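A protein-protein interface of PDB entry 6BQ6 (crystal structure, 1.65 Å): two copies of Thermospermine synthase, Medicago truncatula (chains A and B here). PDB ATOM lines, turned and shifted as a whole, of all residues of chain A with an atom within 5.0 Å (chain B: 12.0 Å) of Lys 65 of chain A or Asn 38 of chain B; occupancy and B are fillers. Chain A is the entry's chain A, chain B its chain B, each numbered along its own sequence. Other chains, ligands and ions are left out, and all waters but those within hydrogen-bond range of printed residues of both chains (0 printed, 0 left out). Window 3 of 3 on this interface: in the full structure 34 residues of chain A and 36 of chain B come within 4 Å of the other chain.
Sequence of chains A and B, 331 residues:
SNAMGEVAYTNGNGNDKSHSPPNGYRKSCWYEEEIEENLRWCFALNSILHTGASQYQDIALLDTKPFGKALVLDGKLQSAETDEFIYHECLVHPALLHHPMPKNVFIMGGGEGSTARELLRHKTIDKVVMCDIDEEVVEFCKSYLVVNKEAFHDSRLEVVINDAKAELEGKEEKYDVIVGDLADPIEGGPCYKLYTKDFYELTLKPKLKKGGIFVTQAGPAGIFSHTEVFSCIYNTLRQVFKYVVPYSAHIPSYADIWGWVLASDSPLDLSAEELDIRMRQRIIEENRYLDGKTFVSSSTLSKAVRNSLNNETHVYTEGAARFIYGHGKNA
The backbone carbonyl oxygen of Cys 42 of chain A sits at hydrogen-bond distance from the backbone NH of Arg 40 of chain B.
O of Asn 38 of chain B sits at hydrogen-bond distance from N of Ala 44 of chain A (2.9 Å).
O of Ala 44 of chain A is in hydrogen-bond range of N of Lys 65 of chain A.
The side-chain amino group (NZ) of Lys 65 of chain A sits at hydrogen-bond distance from the side-chain amide oxygen (OD1) of Asn 46 of chain A (2.8 Å).
N of Phe 67 of chain A sits at hydrogen-bond distance from OG1 of Thr 64 of chain A.
The guanidinium group of Arg 40 of chain B is in salt-bridge range of the side-chain carboxylate of Glu 32 of chain B (3.4 Å).
Glu 37 of chain B touches Trp 30 of chain A (O to CH2, 3.7 Å).
O of Asn 38 of chain B touches CZ3 of Trp 30 of chain A, at 3.6 Å.
CH2 of Trp 30 of chain A touches CD of Arg 40 of chain B, 3.5 Å away.
O of Asn 38 of chain B touches O of Cys 42 of chain A (3.96 Å).
Cys 42 of chain A touches Leu 39 of chain B (O to CA, 3.4 Å).
Phe 43 of chain A touches Asn 38 of chain B (CA to O, 3.6 Å).
Phe 43 of chain A touches Leu 39 of chain B (CD1 to CD1, 3.3 Å).
CB of Lys 65 of chain A touches OD1 of Asn 38 of chain B, at 3.6 Å.
Asn 38 of chain B touches Pro 66 of chain A (O to CG, 3.5 Å).
CD1 of Leu 39 of chain B touches CE2 of Phe 67 of chain A, 3.8 Å away.
Of the printed residues of chain B, Trp 30 of chain A touches Glu 37 (3.7 Å), Asn 38 (3.6 Å) and Arg 40 (3.5 Å).
No residue of chain B comes within 4 Å of Leu 45 of chain A.
No residue of chain B comes within 4 Å of Asn 46 of chain A.
Asp 63 of chain A touches none of the printed residues of chain B.
No residue of chain B comes within 4 Å of Thr 64 of chain A.
Of the printed residues of chain B, Lys 65 of chain A touches Asn 38 (3.6 Å).
Of the printed residues of chain B, Pro 66 of chain A touches Asn 38.
Phe 67 of chain A touches just one residue of chain B: Leu 39.
Glu 33 of chain B touches none of the printed residues of chain A.
Of the printed residues of chain A, Asn 38 of chain B touches Trp 30, Cys 42, Phe 43, Ala 44, Lys 65 and Pro 66.
Trp 41 of chain B touches none of the printed residues of chain A.
The nearest printed residue of chain B that does not touch Lys 65 of chain A is Glu 37 of chain B (6.0 Å).
The nearest printed residue of chain B that does not touch Pro 66 of chain A is Glu 36 of chain B (4.05 Å).
Of the 14 printed residues of chain B, 4 touch a printed residue of chain A.
Hydrophobic or aromatic side chains of chain B that line the printed part of chain A: Leu 39.
Printed residues of chain A that touch a printed residue of chain B: Trp 30, Cys 42, Phe 43, Ala 44, Lys 65, Pro 66 and Phe 67.
Hydrophobic or aromatic side chains of chain A within 4 Å of the printed part of chain B: Trp 30, Phe 43, Ala 44, Pro 66 and Phe 67.
Among the printed residues, 12 pairs touch across the chains.
Among the printed residues, no Asp or Glu carboxylate lies within 4 Å of a Lys or Arg side-chain nitrogen of the other chain.
Position printed for both chains: 42.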
ATOM      1  N   TRP A  30      21.212  19.324 -10.549  1.00  0.00           N
ATOM      2  CA  TRP A  30      20.257  20.438 -10.589  1.00  0.00           C
ATOM      3  C   TRP A  30      18.963  20.106  -9.914  1.00  0.00           C
ATOM      4  O   TRP A  30      18.497  18.960  -9.974  1.00  0.00           O
ATOM      5  CB  TRP A  30      19.964  20.841 -12.057  1.00  0.00           C
ATOM      6  CG  TRP A  30      21.124  21.340 -12.779  1.00  0.00           C
ATOM      7  CD1 TRP A  30      22.053  20.610 -13.467  1.00  0.00           C
ATOM      8  CD2 TRP A  30      21.524  22.700 -12.894  1.00  0.00           C
ATOM      9  NE1 TRP A  30      22.987  21.439 -13.994  1.00  0.00           N
ATOM     10  CE2 TRP A  30      22.674  22.731 -13.662  1.00  0.00           C
ATOM     11  CE3 TRP A  30      21.006  23.918 -12.401  1.00  0.00           C
ATOM     12  CZ2 TRP A  30      23.337  23.924 -13.959  1.00  0.00           C
ATOM     13  CZ3 TRP A  30      21.650  25.080 -12.693  1.00  0.00           C
ATOM     14  CH2 TRP A  30      22.799  25.086 -13.459  1.00  0.00           C
ATOM     15  N   CYS A  42      16.056  26.717 -12.256  1.00  0.00           N
ATOM     16  CA  CYS A  42      16.875  25.575 -11.852  1.00  0.00           C
ATOM     17  C   CYS A  42      18.085  26.071 -11.103  1.00  0.00           C
ATOM     18  O   CYS A  42      18.776  27.000 -11.522  1.00  0.00           O
ATOM     19  CB  CYS A  42      17.329  24.729 -13.034  1.00  0.00           C
ATOM     20  SG  CYS A  42      16.075  24.548 -14.305  1.00  0.00           S
ATOM     21  N   PHE A  43      18.350  25.403  -9.986  1.00  0.00           N
ATOM     22  CA  PHE A  43      19.507  25.682  -9.123  1.00  0.00           C
ATOM     23  C   PHE A  43      20.498  24.525  -9.135  1.00  0.00           C
ATOM     24  O   PHE A  43      20.102  23.401  -8.949  1.00  0.00           O
ATOM     25  CB  PHE A  43      19.086  25.778  -7.641  1.00  0.00           C
ATOM     26  CG  PHE A  43      17.965  26.685  -7.361  1.00  0.00           C
ATOM     27  CD1 PHE A  43      17.738  27.818  -8.125  1.00  0.00           C
ATOM     28  CD2 PHE A  43      17.220  26.508  -6.234  1.00  0.00           C
ATOM     29  CE1 PHE A  43      16.710  28.689  -7.848  1.00  0.00           C
ATOM     30  CE2 PHE A  43      16.167  27.401  -5.923  1.00  0.00           C
ATOM     31  CZ  PHE A  43      15.915  28.489  -6.728  1.00  0.00           C
ATOM     32  N   ALA A  44      21.771  24.816  -9.291  1.00  0.00           N
ATOM     33  CA  ALA A  44      22.800  23.790  -9.102  1.00  0.00           C
ATOM     34  C   ALA A  44      22.847  23.322  -7.633  1.00  0.00           C
ATOM     35  O   ALA A  44      22.619  24.092  -6.683  1.00  0.00           O
ATOM     36  CB  ALA A  44      24.146  24.283  -9.567  1.00  0.00           C
ATOM     37  N   LEU A  45      23.096  22.035  -7.457  1.00  0.00           N
ATOM     38  CA  LEU A  45      23.108  21.390  -6.179  1.00  0.00           C
ATOM     39  C   LEU A  45      24.503  20.991  -5.714  1.00  0.00           C
ATOM     40  O   LEU A  45      25.315  20.478  -6.475  1.00  0.00           O
ATOM     41  CB  LEU A  45      22.282  20.112  -6.230  1.00  0.00           C
ATOM     42  CG  LEU A  45      20.796  20.239  -6.526  1.00  0.00           C
ATOM     43  CD1 LEU A  45      20.229  18.823  -6.468  1.00  0.00           C
ATOM     44  CD2 LEU A  45      20.143  21.169  -5.507  1.00  0.00           C
ATOM     45  N   ASN A  46      24.726  21.160  -4.413  1.00  0.00           N
ATOM     46  CA  ASN A  46      25.841  20.533  -3.687  1.00  0.00           C
ATOM     47  C   ASN A  46      25.436  19.208  -3.137  1.00  0.00           C
ATOM     48  O   ASN A  46      26.208  18.283  -3.207  1.00  0.00           O
ATOM     49  CB  ASN A  46      26.308  21.406  -2.534  1.00  0.00           C
ATOM     50  CG  ASN A  46      26.994  22.660  -3.017  1.00  0.00           C
ATOM     51  OD1 ASN A  46      27.799  22.623  -3.966  1.00  0.00           O
ATOM     52  ND2 ASN A  46      26.700  23.769  -2.380  1.00  0.00           N
ATOM     53  N   ASP A  63      21.010  21.375  -0.471  1.00  0.00           N
ATOM     54  CA  ASP A  63      22.077  22.309  -0.308  1.00  0.00           C
ATOM     55  C   ASP A  63      22.378  22.796  -1.721  1.00  0.00           C
ATOM     56  O   ASP A  63      22.943  22.104  -2.485  1.00  0.00           O
ATOM     57  CB  ASP A  63      23.298  21.664   0.275  1.00  0.00           C
ATOM     58  CG  ASP A  63      24.430  22.639   0.500  1.00  0.00           C
ATOM     59  OD1 ASP A  63      24.513  23.688  -0.101  1.00  0.00           O
ATOM     60  OD2 ASP A  63      25.267  22.334   1.307  1.00  0.00           O
ATOM     61  N   THR A  64      21.960  24.008  -2.010  1.00  0.00           N
ATOM     62  CA  THR A  64      22.047  24.579  -3.331  1.00  0.00           C
ATOM     63  C   THR A  64      23.222  25.526  -3.450  1.00  0.00           C
ATOM     64  O   THR A  64      23.566  26.257  -2.509  1.00  0.00           O
ATOM     65  CB  THR A  64      20.755  25.322  -3.751  1.00  0.00           C
ATOM     66  OG1 THR A  64      20.733  26.644  -3.215  1.00  0.00           O
ATOM     67  CG2 THR A  64      19.545  24.584  -3.315  1.00  0.00           C
ATOM     68  N   LYS A  65      23.777  25.579  -4.655  1.00  0.00           N
ATOM     69  CA  LYS A  65      24.925  26.424  -4.898  1.00  0.00           C
ATOM     70  C   LYS A  65      24.513  27.875  -4.830  1.00  0.00           C
ATOM     71  O   LYS A  65      25.130  28.630  -4.072  1.00  0.00           O
ATOM     72  CB  LYS A  65      25.634  26.073  -6.190  1.00  0.00           C
ATOM     73  CG  LYS A  65      26.448  24.785  -6.047  1.00  0.00           C
ATOM     74  CD  LYS A  65      27.132  24.425  -7.358  1.00  0.00           C
ATOM     75  CE  LYS A  65      27.768  23.052  -7.300  1.00  0.00           C
ATOM     76  NZ  LYS A  65      28.984  23.070  -6.449  1.00  0.00           N
ATOM     77  N   PRO A  66      23.444  28.298  -5.578  1.00  0.00           N
ATOM     78  CA  PRO A  66      23.185  29.747  -5.552  1.00  0.00           C
ATOM     79  C   PRO A  66      22.553  30.311  -4.257  1.00  0.00           C
ATOM     80  O   PRO A  66      22.782  31.463  -3.905  1.00  0.00           O
ATOM     81  CB  PRO A  66      22.217  29.952  -6.740  1.00  0.00           C
ATOM     82  CG  PRO A  66      21.588  28.620  -6.956  1.00  0.00           C
ATOM     83  CD  PRO A  66      22.540  27.570  -6.486  1.00  0.00           C
ATOM     84  N   PHE A  67      21.764  29.518  -3.552  1.00  0.00           N
ATOM     85  CA  PHE A  67      20.951  30.062  -2.460  1.00  0.00           C
ATOM     86  C   PHE A  67      21.128  29.329  -1.115  1.00  0.00           C
ATOM     87  O   PHE A  67      20.355  29.529  -0.162  1.00  0.00           O
ATOM     88  CB  PHE A  67      19.468  30.075  -2.903  1.00  0.00           C
ATOM     89  CG  PHE A  67      19.218  30.923  -4.129  1.00  0.00           C
ATOM     90  CD1 PHE A  67      19.588  32.247  -4.144  1.00  0.00           C
ATOM     91  CD2 PHE A  67      18.662  30.386  -5.270  1.00  0.00           C
ATOM     92  CE1 PHE A  67      19.402  33.065  -5.268  1.00  0.00           C
ATOM     93  CE2 PHE A  67      18.461  31.206  -6.388  1.00  0.00           C
ATOM     94  CZ  PHE A  67      18.817  32.529  -6.386  1.00  0.00           C
ATOM     95  N   GLY A  68      22.149  28.492  -1.009  1.00  0.00           N
ATOM     96  CA  GLY A  68      22.322  27.703   0.194  1.00  0.00           C
ATOM     97  C   GLY A  68      21.240  26.685   0.447  1.00  0.00           C
ATOM     98  O   GLY A  68      20.683  26.131  -0.482  1.00  0.00           O
ATOM     99  N   GLU B  32      16.909  28.222 -22.740  1.00  0.00           N
ATOM    100  CA  GLU B  32      17.565  28.157 -21.459  1.00  0.00           C
ATOM    101  C   GLU B  32      18.668  29.192 -21.428  1.00  0.00           C
ATOM    102  O   GLU B  32      19.458  29.332 -22.351  1.00  0.00           O
ATOM    103  CB  GLU B  32      18.142  26.767 -21.323  1.00  0.00           C
ATOM    104  CG  GLU B  32      19.098  26.561 -20.199  1.00  0.00           C
ATOM    105  CD  GLU B  32      19.653  25.160 -20.303  1.00  0.00           C
ATOM    106  OE1 GLU B  32      20.875  25.082 -20.606  1.00  0.00           O
ATOM    107  OE2 GLU B  32      18.816  24.184 -20.179  1.00  0.00           O
ATOM    108  N   GLU B  33      18.708  29.925 -20.347  1.00  0.00           N
ATOM    109  CA  GLU B  33      19.791  30.829 -20.085  1.00  0.00           C
ATOM    110  C   GLU B  33      20.376  30.589 -18.692  1.00  0.00           C
ATOM    111  O   GLU B  33      19.640  30.455 -17.693  1.00  0.00           O
ATOM    112  CB  GLU B  33      19.325  32.247 -20.197  1.00  0.00           C
ATOM    113  CG  GLU B  33      20.535  33.201 -20.204  1.00  0.00           C
ATOM    114  CD  GLU B  33      20.238  34.609 -20.672  1.00  0.00           C
ATOM    115  OE1 GLU B  33      19.259  34.808 -21.380  1.00  0.00           O
ATOM    116  OE2 GLU B  33      21.015  35.530 -20.355  1.00  0.00           O
ATOM    117  N   GLU B  34      21.702  30.498 -18.681  1.00  0.00           N
ATOM    118  CA  GLU B  34      22.482  30.433 -17.474  1.00  0.00           C
ATOM    119  C   GLU B  34      22.653  31.863 -17.006  1.00  0.00           C
ATOM    120  O   GLU B  34      23.557  32.531 -17.441  1.00  0.00           O
ATOM    121  CB  GLU B  34      23.851  29.773 -17.732  1.00  0.00           C
ATOM    122  CG  GLU B  34      23.775  28.271 -18.070  1.00  0.00           C
ATOM    123  CD  GLU B  34      24.969  27.450 -17.543  1.00  0.00           C
ATOM    124  OE1 GLU B  34      24.733  26.321 -17.039  1.00  0.00           O
ATOM    125  OE2 GLU B  34      26.127  27.937 -17.620  1.00  0.00           O
ATOM    126  N   ILE B  35      21.774  32.311 -16.115  1.00  0.00           N
ATOM    127  CA  ILE B  35      21.918  33.617 -15.440  1.00  0.00           C
ATOM    128  C   ILE B  35      23.287  33.723 -14.732  1.00  0.00           C
ATOM    129  O   ILE B  35      24.002  34.715 -14.883  1.00  0.00           O
ATOM    130  CB  ILE B  35      20.796  33.824 -14.371  1.00  0.00           C
ATOM    131  CG1 ILE B  35      19.393  33.791 -14.992  1.00  0.00           C
ATOM    132  CG2 ILE B  35      21.030  35.112 -13.589  1.00  0.00           C
ATOM    133  CD1 ILE B  35      19.261  34.552 -16.293  1.00  0.00           C
ATOM    134  N   GLU B  36      23.591  32.717 -13.931  1.00  0.00           N
ATOM    135  CA  GLU B  36      24.902  32.527 -13.292  1.00  0.00           C
ATOM    136  C   GLU B  36      25.318  31.118 -13.702  1.00  0.00           C
ATOM    137  O   GLU B  36      24.473  30.333 -14.140  1.00  0.00           O
ATOM    138  CB  GLU B  36      24.769  32.609 -11.765  1.00  0.00           C
ATOM    139  CG  GLU B  36      23.942  33.780 -11.217  1.00  0.00           C
ATOM    140  CD  GLU B  36      23.893  33.872  -9.671  1.00  0.00           C
ATOM    141  OE1 GLU B  36      23.707  35.014  -9.184  1.00  0.00           O
ATOM    142  OE2 GLU B  36      24.013  32.841  -8.929  1.00  0.00           O
ATOM    143  N   GLU B  37      26.578  30.722 -13.512  1.00  0.00           N
ATOM    144  CA  GLU B  37      26.914  29.301 -13.743  1.00  0.00           C
ATOM    145  C   GLU B  37      26.056  28.285 -12.952  1.00  0.00           C
ATOM    146  O   GLU B  37      25.943  27.112 -13.370  1.00  0.00           O
ATOM    147  CB  GLU B  37      28.391  29.014 -13.462  1.00  0.00           C
ATOM    148  CG  GLU B  37      28.843  29.360 -12.088  1.00  0.00           C
ATOM    149  CD  GLU B  37      30.234  28.835 -11.815  1.00  0.00           C
ATOM    150  OE1 GLU B  37      31.136  29.179 -12.612  1.00  0.00           O
ATOM    151  OE2 GLU B  37      30.401  28.096 -10.813  1.00  0.00           O
ATOM    152  N   ASN B  38      25.455  28.720 -11.848  1.00  0.00           N
ATOM    153  CA  ASN B  38      24.673  27.828 -11.007  1.00  0.00           C
ATOM    154  C   ASN B  38      23.175  28.068 -11.000  1.00  0.00           C
ATOM    155  O   ASN B  38      22.463  27.496 -10.167  1.00  0.00           O
ATOM    156  CB  ASN B  38      25.207  27.920  -9.599  1.00  0.00           C
ATOM    157  CG  ASN B  38      26.630  27.416  -9.509  1.00  0.00           C
ATOM    158  OD1 ASN B  38      27.416  27.900  -8.716  1.00  0.00           O
ATOM    159  ND2 ASN B  38      26.967  26.451 -10.369  1.00  0.00           N
ATOM    160  N   LEU B  39      22.706  28.876 -11.930  1.00  0.00           N
ATOM    161  CA  LEU B  39      21.309  29.186 -11.990  1.00  0.00           C
ATOM    162  C   LEU B  39      20.784  29.261 -13.419  1.00  0.00           C
ATOM    163  O   LEU B  39      21.315  29.954 -14.202  1.00  0.00           O
ATOM    164  CB  LEU B  39      21.156  30.530 -11.319  1.00  0.00           C
ATOM    165  CG  LEU B  39      19.839  31.124 -10.973  1.00  0.00           C
ATOM    166  CD1 LEU B  39      19.101  30.225  -9.999  1.00  0.00           C
ATOM    167  CD2 LEU B  39      20.158  32.453 -10.352  1.00  0.00           C
ATOM    168  N   ARG B  40      19.721  28.539 -13.702  1.00  0.00           N
ATOM    169  CA  ARG B  40      19.190  28.506 -15.043  1.00  0.00           C
ATOM    170  C   ARG B  40      17.754  28.950 -15.068  1.00  0.00           C
ATOM    171  O   ARG B  40      16.997  28.632 -14.192  1.00  0.00           O
ATOM    172  CB  ARG B  40      19.373  27.126 -15.651  1.00  0.00           C
ATOM    173  CG  ARG B  40      20.784  26.951 -16.152  1.00  0.00           C
ATOM    174  CD  ARG B  40      21.173  25.533 -16.572  1.00  0.00           C
ATOM    175  NE  ARG B  40      20.022  24.676 -16.786  1.00  0.00           N
ATOM    176  CZ  ARG B  40      20.121  23.372 -17.024  1.00  0.00           C
ATOM    177  NH1 ARG B  40      21.313  22.777 -17.159  1.00  0.00           N
ATOM    178  NH2 ARG B  40      19.005  22.659 -17.189  1.00  0.00           N
ATOM    179  N   TRP B  41      17.414  29.697 -16.094  1.00  0.00           N
ATOM    180  CA  TRP B  41      16.104  30.316 -16.196  1.00  0.00           C
ATOM    181  C   TRP B  41      15.599  29.904 -17.561  1.00  0.00           C
ATOM    182  O   TRP B  41      16.288  30.217 -18.550  1.00  0.00           O
ATOM    183  CB  TRP B  41      16.360  31.801 -16.120  1.00  0.00           C
ATOM    184  CG  TRP B  41      15.284  32.758 -16.217  1.00  0.00           C
ATOM    185  CD1 TRP B  41      15.291  33.900 -16.995  1.00  0.00           C
ATOM    186  CD2 TRP B  41      14.098  32.810 -15.435  1.00  0.00           C
ATOM    187  NE1 TRP B  41      14.176  34.655 -16.720  1.00  0.00           N
ATOM    188  CE2 TRP B  41      13.425  34.006 -15.777  1.00  0.00           C
ATOM    189  CE3 TRP B  41      13.548  31.984 -14.459  1.00  0.00           C
ATOM    190  CZ2 TRP B  41      12.224  34.358 -15.213  1.00  0.00           C
ATOM    191  CZ3 TRP B  41      12.350  32.323 -13.904  1.00  0.00           C
ATOM    192  CH2 TRP B  41      11.682  33.513 -14.292  1.00  0.00           C
ATOM    193  N   CYS B  42      14.467  29.176 -17.624  1.00  0.00           N
ATOM    194  CA  CYS B  42      14.041  28.532 -18.871  1.00  0.00           C
ATOM    195  C   CYS B  42      12.627  28.934 -19.280  1.00  0.00           C
ATOM    196  O   CYS B  42      11.732  28.965 -18.453  1.00  0.00           O
ATOM    197  CB  CYS B  42      14.118  27.030 -18.765  1.00  0.00           C
ATOM    198  SG  CYS B  42      15.666  26.487 -17.951  1.00  0.00           S
ATOM    199  N   PHE B 224      22.050  40.630  -3.598  1.00  0.00           N
ATOM    200  CA  PHE B 224      23.429  40.181  -3.751  1.00  0.00           C
ATOM    201  C   PHE B 224      24.041  40.467  -5.133  1.00  0.00           C
ATOM    202  O   PHE B 224      25.253  40.725  -5.240  1.00  0.00           O
ATOM    203  CB  PHE B 224      23.527  38.703  -3.375  1.00  0.00           C
ATOM    204  CG  PHE B 224      23.065  38.456  -1.974  1.00  0.00           C
ATOM    205  CD1 PHE B 224      23.679  39.122  -0.892  1.00  0.00           C
ATOM    206  CD2 PHE B 224      21.974  37.678  -1.732  1.00  0.00           C
ATOM    207  CE1 PHE B 224      23.235  38.908   0.401  1.00  0.00           C
ATOM    208  CE2 PHE B 224      21.509  37.465  -0.443  1.00  0.00           C
ATOM    209  CZ  PHE B 224      22.117  38.101   0.617  1.00  0.00           C
ATOM    210  N   GLU B 228      28.233  42.915  -8.521  1.00  0.00           N
ATOM    211  CA  GLU B 228      29.083  42.553  -9.674  1.00  0.00           C
ATOM    212  C   GLU B 228      29.425  43.794 -10.472  1.00  0.00           C
ATOM    213  O   GLU B 228      30.555  43.981 -10.848  1.00  0.00           O
ATOM    214  CB  GLU B 228      28.416  41.596 -10.668  1.00  0.00           C
ATOM    215  CG  GLU B 228      27.694  40.342 -10.203  1.00  0.00           C
ATOM    216  CD  GLU B 228      26.643  39.971 -11.259  1.00  0.00           C
ATOM    217  OE1 GLU B 228      25.477  39.690 -10.849  1.00  0.00           O
ATOM    218  OE2 GLU B 228      26.990  40.056 -12.516  1.00  0.00           O
ATOM    219  N   ALA B 255      14.932  37.807 -14.679  1.00  0.00           N
ATOM    220  CA  ALA B 255      15.015  37.116 -13.387  1.00  0.00           C
ATOM    221  C   ALA B 255      15.809  37.871 -12.334  1.00  0.00           C
ATOM    222  O   ALA B 255      16.497  37.270 -11.521  1.00  0.00           O
ATOM    223  CB  ALA B 255      15.565  35.668 -13.536  1.00  0.00           C
